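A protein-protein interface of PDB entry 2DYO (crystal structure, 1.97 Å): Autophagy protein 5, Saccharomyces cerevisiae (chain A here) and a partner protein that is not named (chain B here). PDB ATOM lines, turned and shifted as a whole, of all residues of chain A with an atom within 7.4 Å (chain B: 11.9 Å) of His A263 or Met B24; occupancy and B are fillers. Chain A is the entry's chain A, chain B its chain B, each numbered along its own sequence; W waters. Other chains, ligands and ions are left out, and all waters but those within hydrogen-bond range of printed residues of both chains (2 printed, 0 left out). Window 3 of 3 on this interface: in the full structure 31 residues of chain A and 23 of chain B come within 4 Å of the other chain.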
ATOM      1  N   ILE A   7      -1.779   1.985  -0.027  1.00  0.00           N
ATOM      2  CA  ILE A   7      -1.465   3.146  -0.848  1.00  0.00           C
ATOM      3  C   ILE A   7      -2.451   3.217  -2.013  1.00  0.00           C
ATOM      4  O   ILE A   7      -3.028   4.266  -2.275  1.00  0.00           O
ATOM      5  CB  ILE A   7      -0.016   3.059  -1.396  1.00  0.00           C
ATOM      6  CG1 ILE A   7       0.985   3.227  -0.246  1.00  0.00           C
ATOM      7  CG2 ILE A   7       0.214   4.130  -2.463  1.00  0.00           C
ATOM      8  CD1 ILE A   7       2.437   3.006  -0.646  1.00  0.00           C
ATOM      9  N   PRO A 230      16.615   2.085 -11.521  1.00  0.00           N
ATOM     10  CA  PRO A 230      16.813   3.534 -11.461  1.00  0.00           C
ATOM     11  C   PRO A 230      15.921   4.333 -10.517  1.00  0.00           C
ATOM     12  O   PRO A 230      14.781   3.961 -10.231  1.00  0.00           O
ATOM     13  CB  PRO A 230      16.627   3.966 -12.917  1.00  0.00           C
ATOM     14  CG  PRO A 230      15.595   3.021 -13.408  1.00  0.00           C
ATOM     15  CD  PRO A 230      16.054   1.685 -12.823  1.00  0.00           C
ATOM     16  N   THR A 231      16.474   5.443 -10.044  1.00  0.00           N
ATOM     17  CA  THR A 231      15.769   6.373  -9.179  1.00  0.00           C
ATOM     18  C   THR A 231      15.334   7.495 -10.125  1.00  0.00           C
ATOM     19  O   THR A 231      15.726   7.507 -11.294  1.00  0.00           O
ATOM     20  CB  THR A 231      16.706   6.986  -8.134  1.00  0.00           C
ATOM     21  OG1 THR A 231      17.732   7.721  -8.812  1.00  0.00           O
ATOM     22  CG2 THR A 231      17.353   5.901  -7.278  1.00  0.00           C
ATOM     23  N   LEU A 232      14.524   8.429  -9.641  1.00  0.00           N
ATOM     24  CA  LEU A 232      14.109   9.540 -10.496  1.00  0.00           C
ATOM     25  C   LEU A 232      15.339  10.327 -10.945  1.00  0.00           C
ATOM     26  O   LEU A 232      15.412  10.786 -12.086  1.00  0.00           O
ATOM     27  CB  LEU A 232      13.149  10.468  -9.755  1.00  0.00           C
ATOM     28  CG  LEU A 232      11.730   9.934  -9.536  1.00  0.00           C
ATOM     29  CD1 LEU A 232      10.880  10.998  -8.841  1.00  0.00           C
ATOM     30  CD2 LEU A 232      11.111   9.558 -10.885  1.00  0.00           C
ATOM     31  N   LYS A 233      16.305  10.486 -10.045  1.00  0.00           N
ATOM     32  CA  LYS A 233      17.531  11.213 -10.378  1.00  0.00           C
ATOM     33  C   LYS A 233      18.254  10.515 -11.523  1.00  0.00           C
ATOM     34  O   LYS A 233      18.811  11.166 -12.405  1.00  0.00           O
ATOM     35  CB  LYS A 233      18.460  11.284  -9.166  1.00  0.00           C
ATOM     36  CG  LYS A 233      19.758  12.046  -9.422  1.00  0.00           C
ATOM     37  CD  LYS A 233      19.512  13.550  -9.465  1.00  0.00           C
ATOM     38  CE  LYS A 233      20.823  14.333  -9.560  1.00  0.00           C
ATOM     39  NZ  LYS A 233      20.598  15.793  -9.314  1.00  0.00           N
ATOM     40  N   ASP A 234      18.245   9.188 -11.501  1.00  0.00           N
ATOM     41  CA  ASP A 234      18.892   8.392 -12.538  1.00  0.00           C
ATOM     42  C   ASP A 234      18.332   8.674 -13.931  1.00  0.00           C
ATOM     43  O   ASP A 234      19.028   8.504 -14.933  1.00  0.00           O
ATOM     44  CB  ASP A 234      18.734   6.900 -12.236  1.00  0.00           C
ATOM     45  CG  ASP A 234      19.719   6.403 -11.202  1.00  0.00           C
ATOM     46  OD1 ASP A 234      19.513   5.284 -10.686  1.00  0.00           O
ATOM     47  OD2 ASP A 234      20.702   7.121 -10.916  1.00  0.00           O
ATOM     48  N   GLU A 259       4.439  15.595  -3.546  1.00  0.00           N
ATOM     49  CA  GLU A 259       5.842  15.813  -3.885  1.00  0.00           C
ATOM     50  C   GLU A 259       6.623  14.506  -3.808  1.00  0.00           C
ATOM     51  O   GLU A 259       6.508  13.765  -2.834  1.00  0.00           O
ATOM     52  CB  GLU A 259       6.461  16.831  -2.923  1.00  0.00           C
ATOM     53  CG  GLU A 259       7.882  17.233  -3.288  1.00  0.00           C
ATOM     54  CD  GLU A 259       8.535  18.101  -2.224  1.00  0.00           C
ATOM     55  OE1 GLU A 259       7.860  19.021  -1.714  1.00  0.00           O
ATOM     56  OE2 GLU A 259       9.720  17.865  -1.907  1.00  0.00           O
ATOM     57  N   ILE A 260       7.422  14.226  -4.835  1.00  0.00           N
ATOM     58  CA  ILE A 260       8.214  13.009  -4.870  1.00  0.00           C
ATOM     59  C   ILE A 260       9.710  13.341  -4.808  1.00  0.00           C
ATOM     60  O   ILE A 260      10.208  14.163  -5.581  1.00  0.00           O
ATOM     61  CB  ILE A 260       7.921  12.193  -6.156  1.00  0.00           C
ATOM     62  CG1 ILE A 260       6.417  11.895  -6.264  1.00  0.00           C
ATOM     63  CG2 ILE A 260       8.699  10.893  -6.134  1.00  0.00           C
ATOM     64  CD1 ILE A 260       5.857  11.037  -5.142  1.00  0.00           C
ATOM     65  N   PRO A 261      10.440  12.715  -3.870  1.00  0.00           N
ATOM     66  CA  PRO A 261      11.884  12.937  -3.698  1.00  0.00           C
ATOM     67  C   PRO A 261      12.672  12.391  -4.890  1.00  0.00           C
ATOM     68  O   PRO A 261      12.272  11.397  -5.492  1.00  0.00           O
ATOM     69  CB  PRO A 261      12.211  12.159  -2.421  1.00  0.00           C
ATOM     70  CG  PRO A 261      10.900  12.040  -1.707  1.00  0.00           C
ATOM     71  CD  PRO A 261       9.925  11.808  -2.831  1.00  0.00           C
ATOM     72  N   TRP A 262      13.798  13.021  -5.221  1.00  0.00           N
ATOM     73  CA  TRP A 262      14.609  12.552  -6.342  1.00  0.00           C
ATOM     74  C   TRP A 262      15.200  11.160  -6.130  1.00  0.00           C
ATOM     75  O   TRP A 262      15.482  10.456  -7.099  1.00  0.00           O
ATOM     76  CB  TRP A 262      15.753  13.527  -6.642  1.00  0.00           C
ATOM     77  CG  TRP A 262      15.315  14.779  -7.331  1.00  0.00           C
ATOM     78  CD1 TRP A 262      15.078  15.992  -6.754  1.00  0.00           C
ATOM     79  CD2 TRP A 262      15.037  14.936  -8.729  1.00  0.00           C
ATOM     80  NE1 TRP A 262      14.670  16.899  -7.707  1.00  0.00           N
ATOM     81  CE2 TRP A 262      14.636  16.276  -8.927  1.00  0.00           C
ATOM     82  CE3 TRP A 262      15.089  14.074  -9.835  1.00  0.00           C
ATOM     83  CZ2 TRP A 262      14.286  16.779 -10.188  1.00  0.00           C
ATOM     84  CZ3 TRP A 262      14.743  14.572 -11.091  1.00  0.00           C
ATOM     85  CH2 TRP A 262      14.346  15.915 -11.255  1.00  0.00           C
ATOM     86  N   HIS A 263      15.400  10.756  -4.876  1.00  0.00           N
ATOM     87  CA  HIS A 263      15.972   9.436  -4.624  1.00  0.00           C
ATOM     88  C   HIS A 263      14.943   8.313  -4.731  1.00  0.00           C
ATOM     89  O   HIS A 263      15.278   7.138  -4.595  1.00  0.00           O
ATOM     90  CB  HIS A 263      16.658   9.378  -3.252  1.00  0.00           C
ATOM     91  CG  HIS A 263      15.761   9.712  -2.100  1.00  0.00           C
ATOM     92  ND1 HIS A 263      15.553  11.003  -1.667  1.00  0.00           N
ATOM     93  CD2 HIS A 263      15.043   8.915  -1.270  1.00  0.00           C
ATOM     94  CE1 HIS A 263      14.751  10.989  -0.615  1.00  0.00           C
ATOM     95  NE2 HIS A 263      14.427   9.736  -0.354  1.00  0.00           N
ATOM     96  N   MET A 264      13.688   8.672  -4.973  1.00  0.00           N
ATOM     97  CA  MET A 264      12.641   7.660  -5.103  1.00  0.00           C
ATOM     98  C   MET A 264      12.929   6.720  -6.270  1.00  0.00           C
ATOM     99  O   MET A 264      13.307   7.163  -7.356  1.00  0.00           O
ATOM    100  CB  MET A 264      11.280   8.335  -5.303  1.00  0.00           C
ATOM    101  CG  MET A 264      10.199   7.406  -5.820  1.00  0.00           C
ATOM    102  SD  MET A 264       8.766   7.330  -4.740  1.00  0.00           S
ATOM    103  CE  MET A 264       9.036   5.740  -3.979  1.00  0.00           C
ATOM    104  N   LEU A 265      12.752   5.424  -6.036  1.00  0.00           N
ATOM    105  CA  LEU A 265      12.972   4.401  -7.061  1.00  0.00           C
ATOM    106  C   LEU A 265      11.824   4.418  -8.066  1.00  0.00           C
ATOM    107  O   LEU A 265      10.651   4.389  -7.683  1.00  0.00           O
ATOM    108  CB  LEU A 265      13.056   3.015  -6.419  1.00  0.00           C
ATOM    109  CG  LEU A 265      14.272   2.733  -5.534  1.00  0.00           C
ATOM    110  CD1 LEU A 265      14.073   1.421  -4.769  1.00  0.00           C
ATOM    111  CD2 LEU A 265      15.520   2.666  -6.402  1.00  0.00           C
ATOM    112  N   LEU A 266      12.161   4.451  -9.352  1.00  0.00           N
ATOM    113  CA  LEU A 266      11.154   4.489 -10.407  1.00  0.00           C
ATOM    114  C   LEU A 266      10.210   3.287 -10.391  1.00  0.00           C
ATOM    115  O   LEU A 266       9.008   3.440 -10.597  1.00  0.00           O
ATOM    116  CB  LEU A 266      11.830   4.608 -11.780  1.00  0.00           C
ATOM    117  CG  LEU A 266      10.896   4.863 -12.967  1.00  0.00           C
ATOM    118  CD1 LEU A 266      10.129   6.165 -12.746  1.00  0.00           C
ATOM    119  CD2 LEU A 266      11.714   4.938 -14.255  1.00  0.00           C
ATOM    120  N   ASP A 268       9.281   1.510  -7.839  1.00  0.00           N
ATOM    121  CA  ASP A 268       8.382   1.723  -6.709  1.00  0.00           C
ATOM    122  C   ASP A 268       7.327   2.761  -7.057  1.00  0.00           C
ATOM    123  O   ASP A 268       6.132   2.552  -6.838  1.00  0.00           O
ATOM    124  CB  ASP A 268       9.163   2.206  -5.485  1.00  0.00           C
ATOM    125  CG  ASP A 268       9.557   1.077  -4.567  1.00  0.00           C
ATOM    126  OD1 ASP A 268       8.646   0.393  -4.052  1.00  0.00           O
ATOM    127  OD2 ASP A 268      10.771   0.874  -4.359  1.00  0.00           O
ATOM    128  N   LYS A 272       3.329   1.695  -7.460  1.00  0.00           N
ATOM    129  CA  LYS A 272       2.430   2.191  -6.426  1.00  0.00           C
ATOM    130  C   LYS A 272       1.586   3.403  -6.790  1.00  0.00           C
ATOM    131  O   LYS A 272       0.410   3.479  -6.421  1.00  0.00           O
ATOM    132  CB  LYS A 272       3.239   2.486  -5.159  1.00  0.00           C
ATOM    133  CG  LYS A 272       3.807   1.225  -4.528  1.00  0.00           C
ATOM    134  CD  LYS A 272       4.824   1.524  -3.440  1.00  0.00           C
ATOM    135  CE  LYS A 272       5.306   0.220  -2.807  1.00  0.00           C
ATOM    136  NZ  LYS A 272       6.521   0.403  -1.976  1.00  0.00           N
ATOM    137  N   ASP B  22       9.888   1.316   3.388  1.00  0.00           N
ATOM    138  CA  ASP B  22       8.756   1.449   4.360  1.00  0.00           C
ATOM    139  C   ASP B  22       8.642   2.884   4.849  1.00  0.00           C
ATOM    140  O   ASP B  22       7.541   3.406   5.040  1.00  0.00           O
ATOM    141  CB  ASP B  22       8.943   0.520   5.523  1.00  0.00           C
ATOM    142  N   SER B  23       9.780   3.536   5.057  1.00  0.00           N
ATOM    143  CA  SER B  23       9.773   4.924   5.511  1.00  0.00           C
ATOM    144  C   SER B  23       9.371   5.758   4.305  1.00  0.00           C
ATOM    145  O   SER B  23       8.767   6.822   4.447  1.00  0.00           O
ATOM    146  CB  SER B  23      11.160   5.341   6.007  1.00  0.00           C
ATOM    147  OG  SER B  23      11.110   6.614   6.636  1.00  0.00           O
ATOM    148  N   MET B  24       9.702   5.256   3.115  1.00  0.00           N
ATOM    149  CA  MET B  24       9.334   5.929   1.878  1.00  0.00           C
ATOM    150  C   MET B  24       7.848   5.659   1.699  1.00  0.00           C
ATOM    151  O   MET B  24       7.087   6.541   1.302  1.00  0.00           O
ATOM    152  CB  MET B  24      10.122   5.364   0.693  1.00  0.00           C
ATOM    153  CG  MET B  24       9.735   5.960  -0.663  1.00  0.00           C
ATOM    154  SD  MET B  24      10.017   7.742  -0.812  1.00  0.00           S
ATOM    155  CE  MET B  24      11.685   7.760  -1.474  1.00  0.00           C
ATOM    156  N   ASP B  25       7.444   4.428   2.002  1.00  0.00           N
ATOM    157  CA  ASP B  25       6.043   4.039   1.916  1.00  0.00           C
ATOM    158  C   ASP B  25       5.278   4.827   2.974  1.00  0.00           C
ATOM    159  O   ASP B  25       4.125   5.209   2.767  1.00  0.00           O
ATOM    160  CB  ASP B  25       5.888   2.534   2.167  1.00  0.00           C
ATOM    161  CG  ASP B  25       5.886   1.723   0.883  1.00  0.00           C
ATOM    162  OD1 ASP B  25       6.388   2.226  -0.143  1.00  0.00           O
ATOM    163  OD2 ASP B  25       5.388   0.574   0.901  1.00  0.00           O
ATOM    164  N   ASP B  26       5.930   5.068   4.112  1.00  0.00           N
ATOM    165  CA  ASP B  26       5.312   5.828   5.191  1.00  0.00           C
ATOM    166  C   ASP B  26       5.177   7.276   4.746  1.00  0.00           C
ATOM    167  O   ASP B  26       4.232   7.966   5.122  1.00  0.00           O
ATOM    168  CB  ASP B  26       6.154   5.755   6.472  1.00  0.00           C
ATOM    169  CG  ASP B  26       6.019   4.419   7.191  1.00  0.00           C
ATOM    170  OD1 ASP B  26       4.880   3.927   7.333  1.00  0.00           O
ATOM    171  OD2 ASP B  26       7.050   3.865   7.630  1.00  0.00           O
ATOM    172  N   LEU B  27       6.129   7.734   3.941  1.00  0.00           N
ATOM    173  CA  LEU B  27       6.103   9.097   3.430  1.00  0.00           C
ATOM    174  C   LEU B  27       4.945   9.218   2.439  1.00  0.00           C
ATOM    175  O   LEU B  27       4.201  10.199   2.445  1.00  0.00           O
ATOM    176  CB  LEU B  27       7.437   9.421   2.742  1.00  0.00           C
ATOM    177  CG  LEU B  27       7.623  10.753   2.005  1.00  0.00           C
ATOM    178  CD1 LEU B  27       9.110  11.057   1.876  1.00  0.00           C
ATOM    179  CD2 LEU B  27       6.975  10.684   0.629  1.00  0.00           C
ATOM    180  N   LEU B  28       4.799   8.206   1.591  1.00  0.00           N
ATOM    181  CA  LEU B  28       3.732   8.188   0.596  1.00  0.00           C
ATOM    182  C   LEU B  28       2.364   8.240   1.274  1.00  0.00           C
ATOM    183  O   LEU B  28       1.544   9.109   0.981  1.00  0.00           O
ATOM    184  CB  LEU B  28       3.845   6.922  -0.259  1.00  0.00           C
ATOM    185  CG  LEU B  28       4.457   7.027  -1.663  1.00  0.00           C
ATOM    186  CD1 LEU B  28       5.363   8.246  -1.795  1.00  0.00           C
ATOM    187  CD2 LEU B  28       5.207   5.735  -1.958  1.00  0.00           C
ATOM    188  N   ILE B  29       2.131   7.305   2.186  1.00  0.00           N
ATOM    189  CA  ILE B  29       0.871   7.239   2.909  1.00  0.00           C
ATOM    190  C   ILE B  29       0.549   8.559   3.599  1.00  0.00           C
ATOM    191  O   ILE B  29      -0.574   9.064   3.514  1.00  0.00           O
ATOM    192  CB  ILE B  29       0.908   6.108   3.953  1.00  0.00           C
ATOM    193  CG1 ILE B  29       0.938   4.759   3.234  1.00  0.00           C
ATOM    194  CG2 ILE B  29      -0.294   6.206   4.879  1.00  0.00           C
ATOM    195  CD1 ILE B  29       1.144   3.577   4.146  1.00  0.00           C
ATOM    196  N   ARG B  30       1.539   9.119   4.281  1.00  0.00           N
ATOM    197  CA  ARG B  30       1.351  10.379   4.983  1.00  0.00           C
ATOM    198  C   ARG B  30       0.925  11.498   4.029  1.00  0.00           C
ATOM    199  O   ARG B  30      -0.073  12.183   4.270  1.00  0.00           O
ATOM    200  CB  ARG B  30       2.646  10.742   5.724  1.00  0.00           C
ATOM    201  CG  ARG B  30       2.737  12.172   6.234  1.00  0.00           C
ATOM    202  CD  ARG B  30       3.608  12.249   7.494  1.00  0.00           C
ATOM    203  NE  ARG B  30       4.737  11.314   7.471  1.00  0.00           N
ATOM    204  CZ  ARG B  30       5.804  11.432   6.684  1.00  0.00           C
ATOM    205  NH1 ARG B  30       5.907  12.453   5.843  1.00  0.00           N
ATOM    206  NH2 ARG B  30       6.769  10.522   6.733  1.00  0.00           N
ATOM    207  N   ARG B  31       1.661  11.671   2.933  1.00  0.00           N
ATOM    208  CA  ARG B  31       1.333  12.723   1.981  1.00  0.00           C
ATOM    209  C   ARG B  31       0.021  12.485   1.227  1.00  0.00           C
ATOM    210  O   ARG B  31      -0.707  13.433   0.934  1.00  0.00           O
ATOM    211  CB  ARG B  31       2.492  12.922   0.994  1.00  0.00           C
ATOM    212  CG  ARG B  31       3.738  13.493   1.670  1.00  0.00           C
ATOM    213  CD  ARG B  31       4.900  13.755   0.715  1.00  0.00           C
ATOM    214  NE  ARG B  31       6.050  14.278   1.453  1.00  0.00           N
ATOM    215  CZ  ARG B  31       7.237  14.556   0.921  1.00  0.00           C
ATOM    216  NH1 ARG B  31       7.460  14.367  -0.373  1.00  0.00           N
ATOM    217  NH2 ARG B  31       8.209  15.027   1.694  1.00  0.00           N
ATOM    218  N   LEU B  32      -0.285  11.226   0.924  1.00  0.00           N
ATOM    219  CA  LEU B  32      -1.518  10.901   0.208  1.00  0.00           C
ATOM    220  C   LEU B  32      -2.738  11.071   1.108  1.00  0.00           C
ATOM    221  O   LEU B  32      -3.805  11.489   0.656  1.00  0.00           O
ATOM    222  CB  LEU B  32      -1.453   9.472  -0.329  1.00  0.00           C
ATOM    223  CG  LEU B  32      -0.506   9.287  -1.522  1.00  0.00           C
ATOM    224  CD1 LEU B  32      -0.360   7.813  -1.840  1.00  0.00           C
ATOM    225  CD2 LEU B  32      -1.045  10.057  -2.733  1.00  0.00           C
ATOM    226  N   THR B  33      -2.578  10.743   2.386  1.00  0.00           N
ATOM    227  CA  THR B  33      -3.671  10.882   3.342  1.00  0.00           C
ATOM    228  C   THR B  33      -3.971  12.366   3.521  1.00  0.00           C
ATOM    229  O   THR B  33      -5.133  12.787   3.548  1.00  0.00           O
ATOM    230  CB  THR B  33      -3.297  10.276   4.707  1.00  0.00           C
ATOM    231  OG1 THR B  33      -2.969   8.892   4.538  1.00  0.00           O
ATOM    232  CG2 THR B  33      -4.468  10.396   5.683  1.00  0.00           C
HETATM  233  O   HOH W   1       8.398   3.322  -1.708  1.00  0.00           O
HETATM  234  O   HOH W   2      10.265  15.269  -0.861  1.00  0.00           O
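The backbone carbonyl oxygen (O) of Glu A259 is in hydrogen-bond range of the guanidinium group (NH1) of Arg B31, 2.7 Å away. The side-chain amino group (NZ) of Lys A272 is in salt-bridge range of the side-chain carboxylate (OD1) of Asp B25.
O of Met A264 is in hydrogen-bond range of N of Leu A232. The side-chain carboxylate (OD1) of Asp A268 lies within salt-bridge range of the side-chain amino group (NZ) of Lys A272 (3.0 Å). The side-chain hydroxyl (OG1) of Thr B33 sits at hydrogen-bond distance from the backbone carbonyl oxygen (O) of Ile B29 (2.6 Å).
CD1 of Ile A7 touches CG of Asp B25, 3.98 Å away. Ile A7 touches Ile B29 (CG1 to CG1, 3.8 Å). Leu B32 touches Ile A7. CE of Met B24 touches CD2 of His A263, 3.6 Å away. CE of Met A264 touches CG of Met B24, at 3.4 Å.
His A263 touches one residue of chain B. Met B24 touches two residues of chain A. Leu A232 touches none of the printed residues of chain B. No residue of chain B comes within 4 Å of Pro A261. Met A264 touches one residue of chain B. No residue of chain B comes within 4 Å of Leu A265. Of the printed residues of chain A, Arg B31 touches Glu A259 (2.7 Å). Printed residues of chain B within 4 Å of Ile A7: Asp B25, Ile B29 and Leu B32. Thr B33 touches none of the printed residues of chain A. The nearest residue of chain B that does not touch His A263 is Leu B27 (5.9 Å). The nearest printed residue of chain A that does not touch Arg B31 is Pro A261 (4.3 Å).
Of the 16 printed residues of chain A, 5 touch a printed residue of chain B. Printed residues of chain B that touch a printed residue of chain A: Met B24, Asp B25, Ile B29, Arg B31 and Leu B32. Along chain B the printed residues that touch a printed residue of chain A span positions 24 to 32. Among the printed residues, Asp or Glu carboxylates within 4 Å of a Lys or Arg side-chain nitrogen of the other chain: Lys A272 with Asp B25 (2.6 Å).
Water W1 bridges the side-chain carboxylate of Asp B25 (2.8 Å) and the side-chain amino group of Lys A272 (3.5 Å). Water W2 bridges the side-chain carboxylate of Glu A259 (2.9 Å) and the guanidinium group of Arg B31 (3.0 Å).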
